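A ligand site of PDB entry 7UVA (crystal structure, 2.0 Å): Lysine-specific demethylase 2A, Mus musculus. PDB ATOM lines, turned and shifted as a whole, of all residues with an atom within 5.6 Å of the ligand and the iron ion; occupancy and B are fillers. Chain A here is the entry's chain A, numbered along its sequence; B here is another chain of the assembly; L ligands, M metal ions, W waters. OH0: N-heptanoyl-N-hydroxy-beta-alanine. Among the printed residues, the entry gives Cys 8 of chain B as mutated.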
ATOM      1  N   ASN A 108      18.875 -15.870   2.759  1.00  0.00           N
ATOM      2  CA  ASN A 108      20.204 -15.885   2.221  1.00  0.00           C
ATOM      3  C   ASN A 108      21.083 -14.890   2.976  1.00  0.00           C
ATOM      4  O   ASN A 108      20.605 -13.803   3.320  1.00  0.00           O
ATOM      5  CB  ASN A 108      20.085 -15.470   0.712  1.00  0.00           C
ATOM      6  CG  ASN A 108      21.278 -15.844  -0.111  1.00  0.00           C
ATOM      7  OD1 ASN A 108      22.199 -16.521   0.355  1.00  0.00           O
ATOM      8  ND2 ASN A 108      21.244 -15.467  -1.397  1.00  0.00           N
ATOM      9  N   ILE A 110      24.347 -12.762   2.354  1.00  0.00           N
ATOM     10  CA  ILE A 110      25.281 -12.324   1.332  1.00  0.00           C
ATOM     11  C   ILE A 110      26.191 -11.147   1.753  1.00  0.00           C
ATOM     12  O   ILE A 110      26.979 -10.678   0.952  1.00  0.00           O
ATOM     13  CB  ILE A 110      24.589 -11.993  -0.009  1.00  0.00           C
ATOM     14  CG1 ILE A 110      23.566 -10.883   0.112  1.00  0.00           C
ATOM     15  CG2 ILE A 110      24.026 -13.268  -0.648  1.00  0.00           C
ATOM     16  CD1 ILE A 110      23.130 -10.334  -1.237  1.00  0.00           C
ATOM     17  N   SER A 111      26.171 -10.779   3.023  1.00  0.00           N
ATOM     18  CA  SER A 111      26.750  -9.552   3.414  1.00  0.00           C
ATOM     19  C   SER A 111      27.515  -9.586   4.745  1.00  0.00           C
ATOM     20  O   SER A 111      27.646  -8.565   5.446  1.00  0.00           O
ATOM     21  CB  SER A 111      25.631  -8.522   3.410  1.00  0.00           C
ATOM     22  OG  SER A 111      26.229  -7.298   3.689  1.00  0.00           O
ATOM     23  N   TYR A 165      33.976 -11.042   2.529  1.00  0.00           N
ATOM     24  CA  TYR A 165      32.624 -11.381   2.866  1.00  0.00           C
ATOM     25  C   TYR A 165      32.470 -12.899   2.796  1.00  0.00           C
ATOM     26  O   TYR A 165      33.161 -13.576   2.054  1.00  0.00           O
ATOM     27  CB  TYR A 165      31.603 -10.754   1.946  1.00  0.00           C
ATOM     28  CG  TYR A 165      31.433  -9.255   2.050  1.00  0.00           C
ATOM     29  CD1 TYR A 165      32.234  -8.365   1.306  1.00  0.00           C
ATOM     30  CD2 TYR A 165      30.373  -8.714   2.774  1.00  0.00           C
ATOM     31  CE1 TYR A 165      32.033  -6.995   1.387  1.00  0.00           C
ATOM     32  CE2 TYR A 165      30.187  -7.325   2.816  1.00  0.00           C
ATOM     33  CZ  TYR A 165      31.022  -6.487   2.145  1.00  0.00           C
ATOM     34  OH  TYR A 165      30.801  -5.116   2.267  1.00  0.00           O
ATOM     35  N   LEU A 167      29.437 -15.616   2.334  1.00  0.00           N
ATOM     36  CA  LEU A 167      28.097 -15.772   1.875  1.00  0.00           C
ATOM     37  C   LEU A 167      27.645 -17.174   2.144  1.00  0.00           C
ATOM     38  O   LEU A 167      28.361 -18.131   1.873  1.00  0.00           O
ATOM     39  CB  LEU A 167      27.947 -15.572   0.374  1.00  0.00           C
ATOM     40  CG  LEU A 167      28.730 -14.567  -0.418  1.00  0.00           C
ATOM     41  CD1 LEU A 167      28.062 -14.508  -1.770  1.00  0.00           C
ATOM     42  CD2 LEU A 167      28.738 -13.205   0.217  1.00  0.00           C
ATOM     43  N   SER A 169      24.312 -19.666   1.721  1.00  0.00           N
ATOM     44  CA  SER A 169      23.125 -19.671   0.909  1.00  0.00           C
ATOM     45  C   SER A 169      22.587 -21.081   0.909  1.00  0.00           C
ATOM     46  O   SER A 169      23.322 -22.032   0.628  1.00  0.00           O
ATOM     47  CB  SER A 169      23.415 -19.198  -0.542  1.00  0.00           C
ATOM     48  OG  SER A 169      24.087 -17.924  -0.614  1.00  0.00           O
ATOM     49  N   TYR A 174      17.831 -17.106  -4.391  1.00  0.00           N
ATOM     50  CA  TYR A 174      17.991 -16.322  -5.590  1.00  0.00           C
ATOM     51  C   TYR A 174      18.196 -14.863  -5.196  1.00  0.00           C
ATOM     52  O   TYR A 174      17.472 -14.341  -4.339  1.00  0.00           O
ATOM     53  CB  TYR A 174      16.738 -16.448  -6.472  1.00  0.00           C
ATOM     54  CG  TYR A 174      16.686 -15.509  -7.655  1.00  0.00           C
ATOM     55  CD1 TYR A 174      17.451 -15.751  -8.765  1.00  0.00           C
ATOM     56  CD2 TYR A 174      15.865 -14.349  -7.639  1.00  0.00           C
ATOM     57  CE1 TYR A 174      17.402 -14.904  -9.867  1.00  0.00           C
ATOM     58  CE2 TYR A 174      15.818 -13.512  -8.732  1.00  0.00           C
ATOM     59  CZ  TYR A 174      16.593 -13.795  -9.837  1.00  0.00           C
ATOM     60  OH  TYR A 174      16.582 -12.931 -10.919  1.00  0.00           O
ATOM     61  N   THR A 175      19.216 -14.230  -5.788  1.00  0.00           N
ATOM     62  CA  THR A 175      19.479 -12.776  -5.659  1.00  0.00           C
ATOM     63  C   THR A 175      19.166 -12.142  -7.054  1.00  0.00           C
ATOM     64  O   THR A 175      19.749 -12.521  -8.081  1.00  0.00           O
ATOM     65  CB  THR A 175      20.961 -12.534  -5.288  1.00  0.00           C
ATOM     66  OG1 THR A 175      21.278 -13.242  -4.052  1.00  0.00           O
ATOM     67  CG2 THR A 175      21.256 -10.996  -5.121  1.00  0.00           C
ATOM     68  N   HIS A 178      21.458  -7.099 -10.208  1.00  0.00           N
ATOM     69  CA  HIS A 178      21.999  -5.902  -9.566  1.00  0.00           C
ATOM     70  C   HIS A 178      23.387  -5.644 -10.096  1.00  0.00           C
ATOM     71  O   HIS A 178      24.006  -6.529 -10.727  1.00  0.00           O
ATOM     72  CB  HIS A 178      22.037  -6.060  -8.024  1.00  0.00           C
ATOM     73  CG  HIS A 178      22.926  -7.167  -7.584  1.00  0.00           C
ATOM     74  ND1 HIS A 178      22.511  -8.487  -7.570  1.00  0.00           N
ATOM     75  CD2 HIS A 178      24.232  -7.181  -7.234  1.00  0.00           C
ATOM     76  CE1 HIS A 178      23.515  -9.265  -7.220  1.00  0.00           C
ATOM     77  NE2 HIS A 178      24.573  -8.506  -6.994  1.00  0.00           N
ATOM     78  N   VAL A 179      23.889  -4.485  -9.729  1.00  0.00           N
ATOM     79  CA  VAL A 179      25.290  -4.123  -9.905  1.00  0.00           C
ATOM     80  C   VAL A 179      25.911  -3.931  -8.493  1.00  0.00           C
ATOM     81  O   VAL A 179      25.360  -3.275  -7.639  1.00  0.00           O
ATOM     82  CB  VAL A 179      25.419  -2.886 -10.801  1.00  0.00           C
ATOM     83  CG1 VAL A 179      26.878  -2.508 -10.999  1.00  0.00           C
ATOM     84  CG2 VAL A 179      24.767  -3.112 -12.156  1.00  0.00           C
ATOM     85  N   ASP A 180      27.071  -4.512  -8.279  1.00  0.00           N
ATOM     86  CA  ASP A 180      27.713  -4.460  -6.953  1.00  0.00           C
ATOM     87  C   ASP A 180      28.012  -3.013  -6.616  1.00  0.00           C
ATOM     88  O   ASP A 180      28.155  -2.177  -7.516  1.00  0.00           O
ATOM     89  CB  ASP A 180      28.967  -5.281  -6.962  1.00  0.00           C
ATOM     90  CG  ASP A 180      28.641  -6.775  -7.133  1.00  0.00           C
ATOM     91  OD1 ASP A 180      27.511  -7.181  -6.753  1.00  0.00           O
ATOM     92  OD2 ASP A 180      29.463  -7.514  -7.717  1.00  0.00           O
ATOM     93  N   PHE A 181      28.022  -2.725  -5.315  1.00  0.00           N
ATOM     94  CA  PHE A 181      28.057  -1.329  -4.900  1.00  0.00           C
ATOM     95  C   PHE A 181      29.289  -0.537  -5.363  1.00  0.00           C
ATOM     96  O   PHE A 181      30.389  -1.065  -5.443  1.00  0.00           O
ATOM     97  CB  PHE A 181      27.769  -1.198  -3.391  1.00  0.00           C
ATOM     98  CG  PHE A 181      28.631  -2.023  -2.516  1.00  0.00           C
ATOM     99  CD1 PHE A 181      30.015  -1.879  -2.544  1.00  0.00           C
ATOM    100  CD2 PHE A 181      28.062  -2.786  -1.516  1.00  0.00           C
ATOM    101  CE1 PHE A 181      30.835  -2.612  -1.657  1.00  0.00           C
ATOM    102  CE2 PHE A 181      28.842  -3.479  -0.602  1.00  0.00           C
ATOM    103  CZ  PHE A 181      30.245  -3.419  -0.671  1.00  0.00           C
ATOM    104  N   VAL A 186      34.461  -7.693  -8.212  1.00  0.00           N
ATOM    105  CA  VAL A 186      34.202  -8.675  -7.191  1.00  0.00           C
ATOM    106  C   VAL A 186      35.015  -9.919  -7.548  1.00  0.00           C
ATOM    107  O   VAL A 186      35.124 -10.259  -8.709  1.00  0.00           O
ATOM    108  CB  VAL A 186      32.685  -8.987  -7.054  1.00  0.00           C
ATOM    109  CG1 VAL A 186      32.354 -10.248  -6.262  1.00  0.00           C
ATOM    110  CG2 VAL A 186      32.009  -7.852  -6.302  1.00  0.00           C
ATOM    111  N   TYR A 188      35.084 -13.980  -6.189  1.00  0.00           N
ATOM    112  CA  TYR A 188      34.029 -14.808  -5.597  1.00  0.00           C
ATOM    113  C   TYR A 188      34.524 -16.292  -5.704  1.00  0.00           C
ATOM    114  O   TYR A 188      34.764 -16.786  -6.788  1.00  0.00           O
ATOM    115  CB  TYR A 188      32.779 -14.511  -6.453  1.00  0.00           C
ATOM    116  CG  TYR A 188      31.444 -15.042  -6.036  1.00  0.00           C
ATOM    117  CD1 TYR A 188      31.039 -16.311  -6.430  1.00  0.00           C
ATOM    118  CD2 TYR A 188      30.525 -14.240  -5.401  1.00  0.00           C
ATOM    119  CE1 TYR A 188      29.773 -16.794  -6.102  1.00  0.00           C
ATOM    120  CE2 TYR A 188      29.264 -14.742  -5.075  1.00  0.00           C
ATOM    121  CZ  TYR A 188      28.878 -16.007  -5.459  1.00  0.00           C
ATOM    122  OH  TYR A 188      27.625 -16.546  -5.159  1.00  0.00           O
ATOM    123  N   LYS A 195      26.847 -22.258  -7.670  1.00  0.00           N
ATOM    124  CA  LYS A 195      26.029 -21.092  -7.956  1.00  0.00           C
ATOM    125  C   LYS A 195      25.798 -21.030  -9.499  1.00  0.00           C
ATOM    126  O   LYS A 195      26.619 -21.477 -10.272  1.00  0.00           O
ATOM    127  CB  LYS A 195      26.805 -19.823  -7.529  1.00  0.00           C
ATOM    128  CG  LYS A 195      27.022 -19.656  -6.019  1.00  0.00           C
ATOM    129  CD  LYS A 195      25.800 -19.007  -5.387  1.00  0.00           C
ATOM    130  CE  LYS A 195      25.852 -18.832  -3.839  1.00  0.00           C
ATOM    131  NZ  LYS A 195      24.831 -17.794  -3.464  1.00  0.00           N
ATOM    132  N   PHE A 197      24.962 -18.019 -12.309  1.00  0.00           N
ATOM    133  CA  PHE A 197      24.936 -16.589 -12.542  1.00  0.00           C
ATOM    134  C   PHE A 197      24.299 -16.323 -13.923  1.00  0.00           C
ATOM    135  O   PHE A 197      24.557 -17.056 -14.872  1.00  0.00           O
ATOM    136  CB  PHE A 197      26.350 -16.008 -12.543  1.00  0.00           C
ATOM    137  CG  PHE A 197      26.908 -15.689 -11.194  1.00  0.00           C
ATOM    138  CD1 PHE A 197      27.313 -16.712 -10.339  1.00  0.00           C
ATOM    139  CD2 PHE A 197      27.128 -14.381 -10.807  1.00  0.00           C
ATOM    140  CE1 PHE A 197      27.860 -16.444  -9.106  1.00  0.00           C
ATOM    141  CE2 PHE A 197      27.682 -14.093  -9.552  1.00  0.00           C
ATOM    142  CZ  PHE A 197      28.054 -15.110  -8.726  1.00  0.00           C
ATOM    143  N   ILE A 244      34.398 -10.589 -11.391  1.00  0.00           N
ATOM    144  CA  ILE A 244      33.318  -9.869 -12.086  1.00  0.00           C
ATOM    145  C   ILE A 244      33.802  -8.416 -12.210  1.00  0.00           C
ATOM    146  O   ILE A 244      34.133  -7.820 -11.192  1.00  0.00           O
ATOM    147  CB  ILE A 244      31.993  -9.852 -11.307  1.00  0.00           C
ATOM    148  CG1 ILE A 244      31.583 -11.249 -10.910  1.00  0.00           C
ATOM    149  CG2 ILE A 244      30.903  -9.232 -12.135  1.00  0.00           C
ATOM    150  CD1 ILE A 244      30.322 -11.320 -10.053  1.00  0.00           C
ATOM    151  N   HIS A 250      24.029  -8.659 -12.807  1.00  0.00           N
ATOM    152  CA  HIS A 250      24.064 -10.084 -12.595  1.00  0.00           C
ATOM    153  C   HIS A 250      23.052 -10.494 -11.525  1.00  0.00           C
ATOM    154  O   HIS A 250      22.675  -9.696 -10.653  1.00  0.00           O
ATOM    155  CB  HIS A 250      25.503 -10.576 -12.313  1.00  0.00           C
ATOM    156  CG  HIS A 250      26.123  -9.967 -11.106  1.00  0.00           C
ATOM    157  ND1 HIS A 250      26.652  -8.694 -11.101  1.00  0.00           N
ATOM    158  CD2 HIS A 250      26.211 -10.402  -9.829  1.00  0.00           C
ATOM    159  CE1 HIS A 250      27.099  -8.394  -9.900  1.00  0.00           C
ATOM    160  NE2 HIS A 250      26.797  -9.390  -9.100  1.00  0.00           N
ATOM    161  N   VAL A 252      21.808 -14.326  -9.405  1.00  0.00           N
ATOM    162  CA  VAL A 252      22.415 -15.495  -8.908  1.00  0.00           C
ATOM    163  C   VAL A 252      21.392 -16.456  -8.272  1.00  0.00           C
ATOM    164  O   VAL A 252      20.599 -16.074  -7.417  1.00  0.00           O
ATOM    165  CB  VAL A 252      23.432 -15.139  -7.828  1.00  0.00           C
ATOM    166  CG1 VAL A 252      24.235 -16.368  -7.488  1.00  0.00           C
ATOM    167  CG2 VAL A 252      24.401 -14.074  -8.329  1.00  0.00           C
ATOM    168  N   THR A 254      21.129 -20.367  -6.317  1.00  0.00           N
ATOM    169  CA  THR A 254      21.852 -21.307  -5.528  1.00  0.00           C
ATOM    170  C   THR A 254      21.199 -22.719  -5.644  1.00  0.00           C
ATOM    171  O   THR A 254      20.159 -22.964  -5.049  1.00  0.00           O
ATOM    172  CB  THR A 254      21.848 -20.858  -4.038  1.00  0.00           C
ATOM    173  OG1 THR A 254      22.346 -19.532  -3.944  1.00  0.00           O
ATOM    174  CG2 THR A 254      22.746 -21.800  -3.237  1.00  0.00           C
ATOM    175  N   GLY A 262      34.293 -14.124  -0.769  1.00  0.00           N
ATOM    176  CA  GLY A 262      34.481 -13.192  -1.853  1.00  0.00           C
ATOM    177  C   GLY A 262      34.685 -11.796  -1.285  1.00  0.00           C
ATOM    178  O   GLY A 262      34.766 -11.604  -0.069  1.00  0.00           O
ATOM    179  N   GLY A 263      34.783 -10.818  -2.158  1.00  0.00           N
ATOM    180  CA  GLY A 263      35.033  -9.456  -1.726  1.00  0.00           C
ATOM    181  C   GLY A 263      35.065  -8.479  -2.888  1.00  0.00           C
ATOM    182  O   GLY A 263      35.070  -8.860  -4.079  1.00  0.00           O
ATOM    183  N   ASN A 264      35.100  -7.213  -2.518  1.00  0.00           N
ATOM    184  CA  ASN A 264      34.849  -6.106  -3.421  1.00  0.00           C
ATOM    185  C   ASN A 264      36.100  -5.318  -3.482  1.00  0.00           C
ATOM    186  O   ASN A 264      36.852  -5.329  -2.531  1.00  0.00           O
ATOM    187  CB  ASN A 264      33.646  -5.208  -3.013  1.00  0.00           C
ATOM    188  CG  ASN A 264      32.339  -5.981  -3.017  1.00  0.00           C
ATOM    189  OD1 ASN A 264      32.171  -6.887  -2.194  1.00  0.00           O
ATOM    190  ND2 ASN A 264      31.409  -5.648  -3.904  1.00  0.00           N
ATOM    191  N   CYS B   8      25.655  -5.580   1.137  1.00  0.00           N
ATOM    192  CA  CYS B   8      25.344  -6.113  -0.187  1.00  0.00           C
ATOM    193  C   CYS B   8      23.886  -6.599  -0.203  1.00  0.00           C
ATOM    194  O   CYS B   8      23.537  -7.482   0.591  1.00  0.00           O
ATOM    195  CB  CYS B   8      26.278  -7.295  -0.483  1.00  0.00           C
ATOM    196  SG  CYS B   8      27.982  -6.802  -0.387  1.00  0.00           S
HETATM  197  C4  OH0 L   1      28.717 -11.204  -3.166  1.00  0.00           C
HETATM  198  C2  OH0 L   1      30.419  -9.630  -2.175  1.00  0.00           C
HETATM  199  O2  OH0 L   1      25.460 -15.361  -4.211  1.00  0.00           O
HETATM  200  C5  OH0 L   1      27.235 -10.754  -3.017  1.00  0.00           C
HETATM  201  C6  OH0 L   1      26.693 -10.454  -4.398  1.00  0.00           C
HETATM  202  N   OH0 L   1      26.368 -11.450  -5.259  1.00  0.00           N
HETATM  203  C   OH0 L   1      28.859  -7.659  -1.671  1.00  0.00           C
HETATM  204  O   OH0 L   1      26.236 -11.139  -6.619  1.00  0.00           O
HETATM  205  C1  OH0 L   1      29.431  -8.981  -1.180  1.00  0.00           C
HETATM  206  C3  OH0 L   1      29.762 -10.135  -3.459  1.00  0.00           C
HETATM  207  C7  OH0 L   1      26.219 -12.868  -4.946  1.00  0.00           C
HETATM  208  C8  OH0 L   1      24.738 -13.101  -4.631  1.00  0.00           C
HETATM  209  C9  OH0 L   1      24.516 -14.550  -4.207  1.00  0.00           C
HETATM  210  O1  OH0 L   1      23.269 -14.942  -3.911  1.00  0.00           O
HETATM  211  O3  OH0 L   1      26.650  -9.260  -4.687  1.00  0.00           O
HETATM  212 FE    FE M   1      26.674  -9.161  -6.893  1.00  0.00          FE
HETATM  213  O   HOH W   1      21.583 -16.953  -4.670  1.00  0.00           O
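Ile 110 touches the ligand.
Tyr 165 touches the ligand (CD1 to C1, 3.8 Å).
Leu 167 touches the ligand.
CG1 of Val 186 touches C3 of the ligand, at 3.8 Å.
Val 252 touches the ligand.
Asn 264 touches the ligand.
Hydrophobic or aromatic side chains within 4 Å of the ligand: Ile 110, Tyr 165, Leu 167, His 178, Val 186, Tyr 188, His 250 and Val 252.
Of the 24 residues printed, 14 come within 4 Å of the ligand.
Water W1 lies within hydrogen-bond range of an oxygen (O1) of the ligand, the side-chain hydroxyl (OG1) of Thr 254 and the backbone carbonyl oxygen (O) of Val 252.
The backbone carbonyl oxygen (O) of Gly 262 sits at hydrogen-bond distance from the backbone NH (N) of Tyr 165, 2.8 Å away.
The backbone carbonyl oxygen of Val 186 sits at hydrogen-bond distance from the backbone NH of Ile 244 (2.8 Å).
N of Cys 8 of chain B lies within hydrogen-bond range of OG of Ser 111.
The side-chain hydroxyl (OG) of Ser 169 lies within hydrogen-bond range of the side-chain amide oxygen (OD1) of Asn 108, at 2.5 Å.
NZ of Lys 195 lies within hydrogen-bond range of OG1 of Thr 254, 3.1 Å away.
O of Val 252 sits at hydrogen-bond distance from N of Thr 175 (2.8 Å).
The side-chain amino group (NZ) of Lys 195 sits at hydrogen-bond distance from the side-chain hydroxyl (OG) of Ser 169.
OG1 of Thr 175 sits at hydrogen-bond distance from ND2 of Asn 108 (3.5 Å).
The iron ion is bound by O of the ligand, at 2.0 Å.
The iron ion is bound by OD1 of Asp 180 (2.2 Å).
The iron ion is bound by a ring nitrogen (NE2) of His 178 (2.2 Å).
The iron ion is bound by O3 of the ligand, at 2.2 Å.
NE2 of His 250 binds the iron ion, 2.2 Å away.
The iron ion has five donor atoms within binding distance.
Three residues have an atom within 4 Å of the iron ion: His 178, Asp 180 and His 250.
The side-chain hydroxyl of Thr 175 is in hydrogen-bond range of an oxygen (O1) of the ligand, at 2.6 Å.
The side-chain hydroxyl (OH) of Tyr 188 sits at hydrogen-bond distance from an oxygen (O2) of the ligand, 2.6 Å away.
The side-chain amide nitrogen (ND2) of Asn 108 is in hydrogen-bond range of an oxygen (O1) of the ligand (3.3 Å).
An oxygen (O2) of the ligand is in salt-bridge range of the side-chain amino group of Lys 195 (2.6 Å).
SG of Cys 8 of chain B is bonded to C of the ligand, 1.8 Å away.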
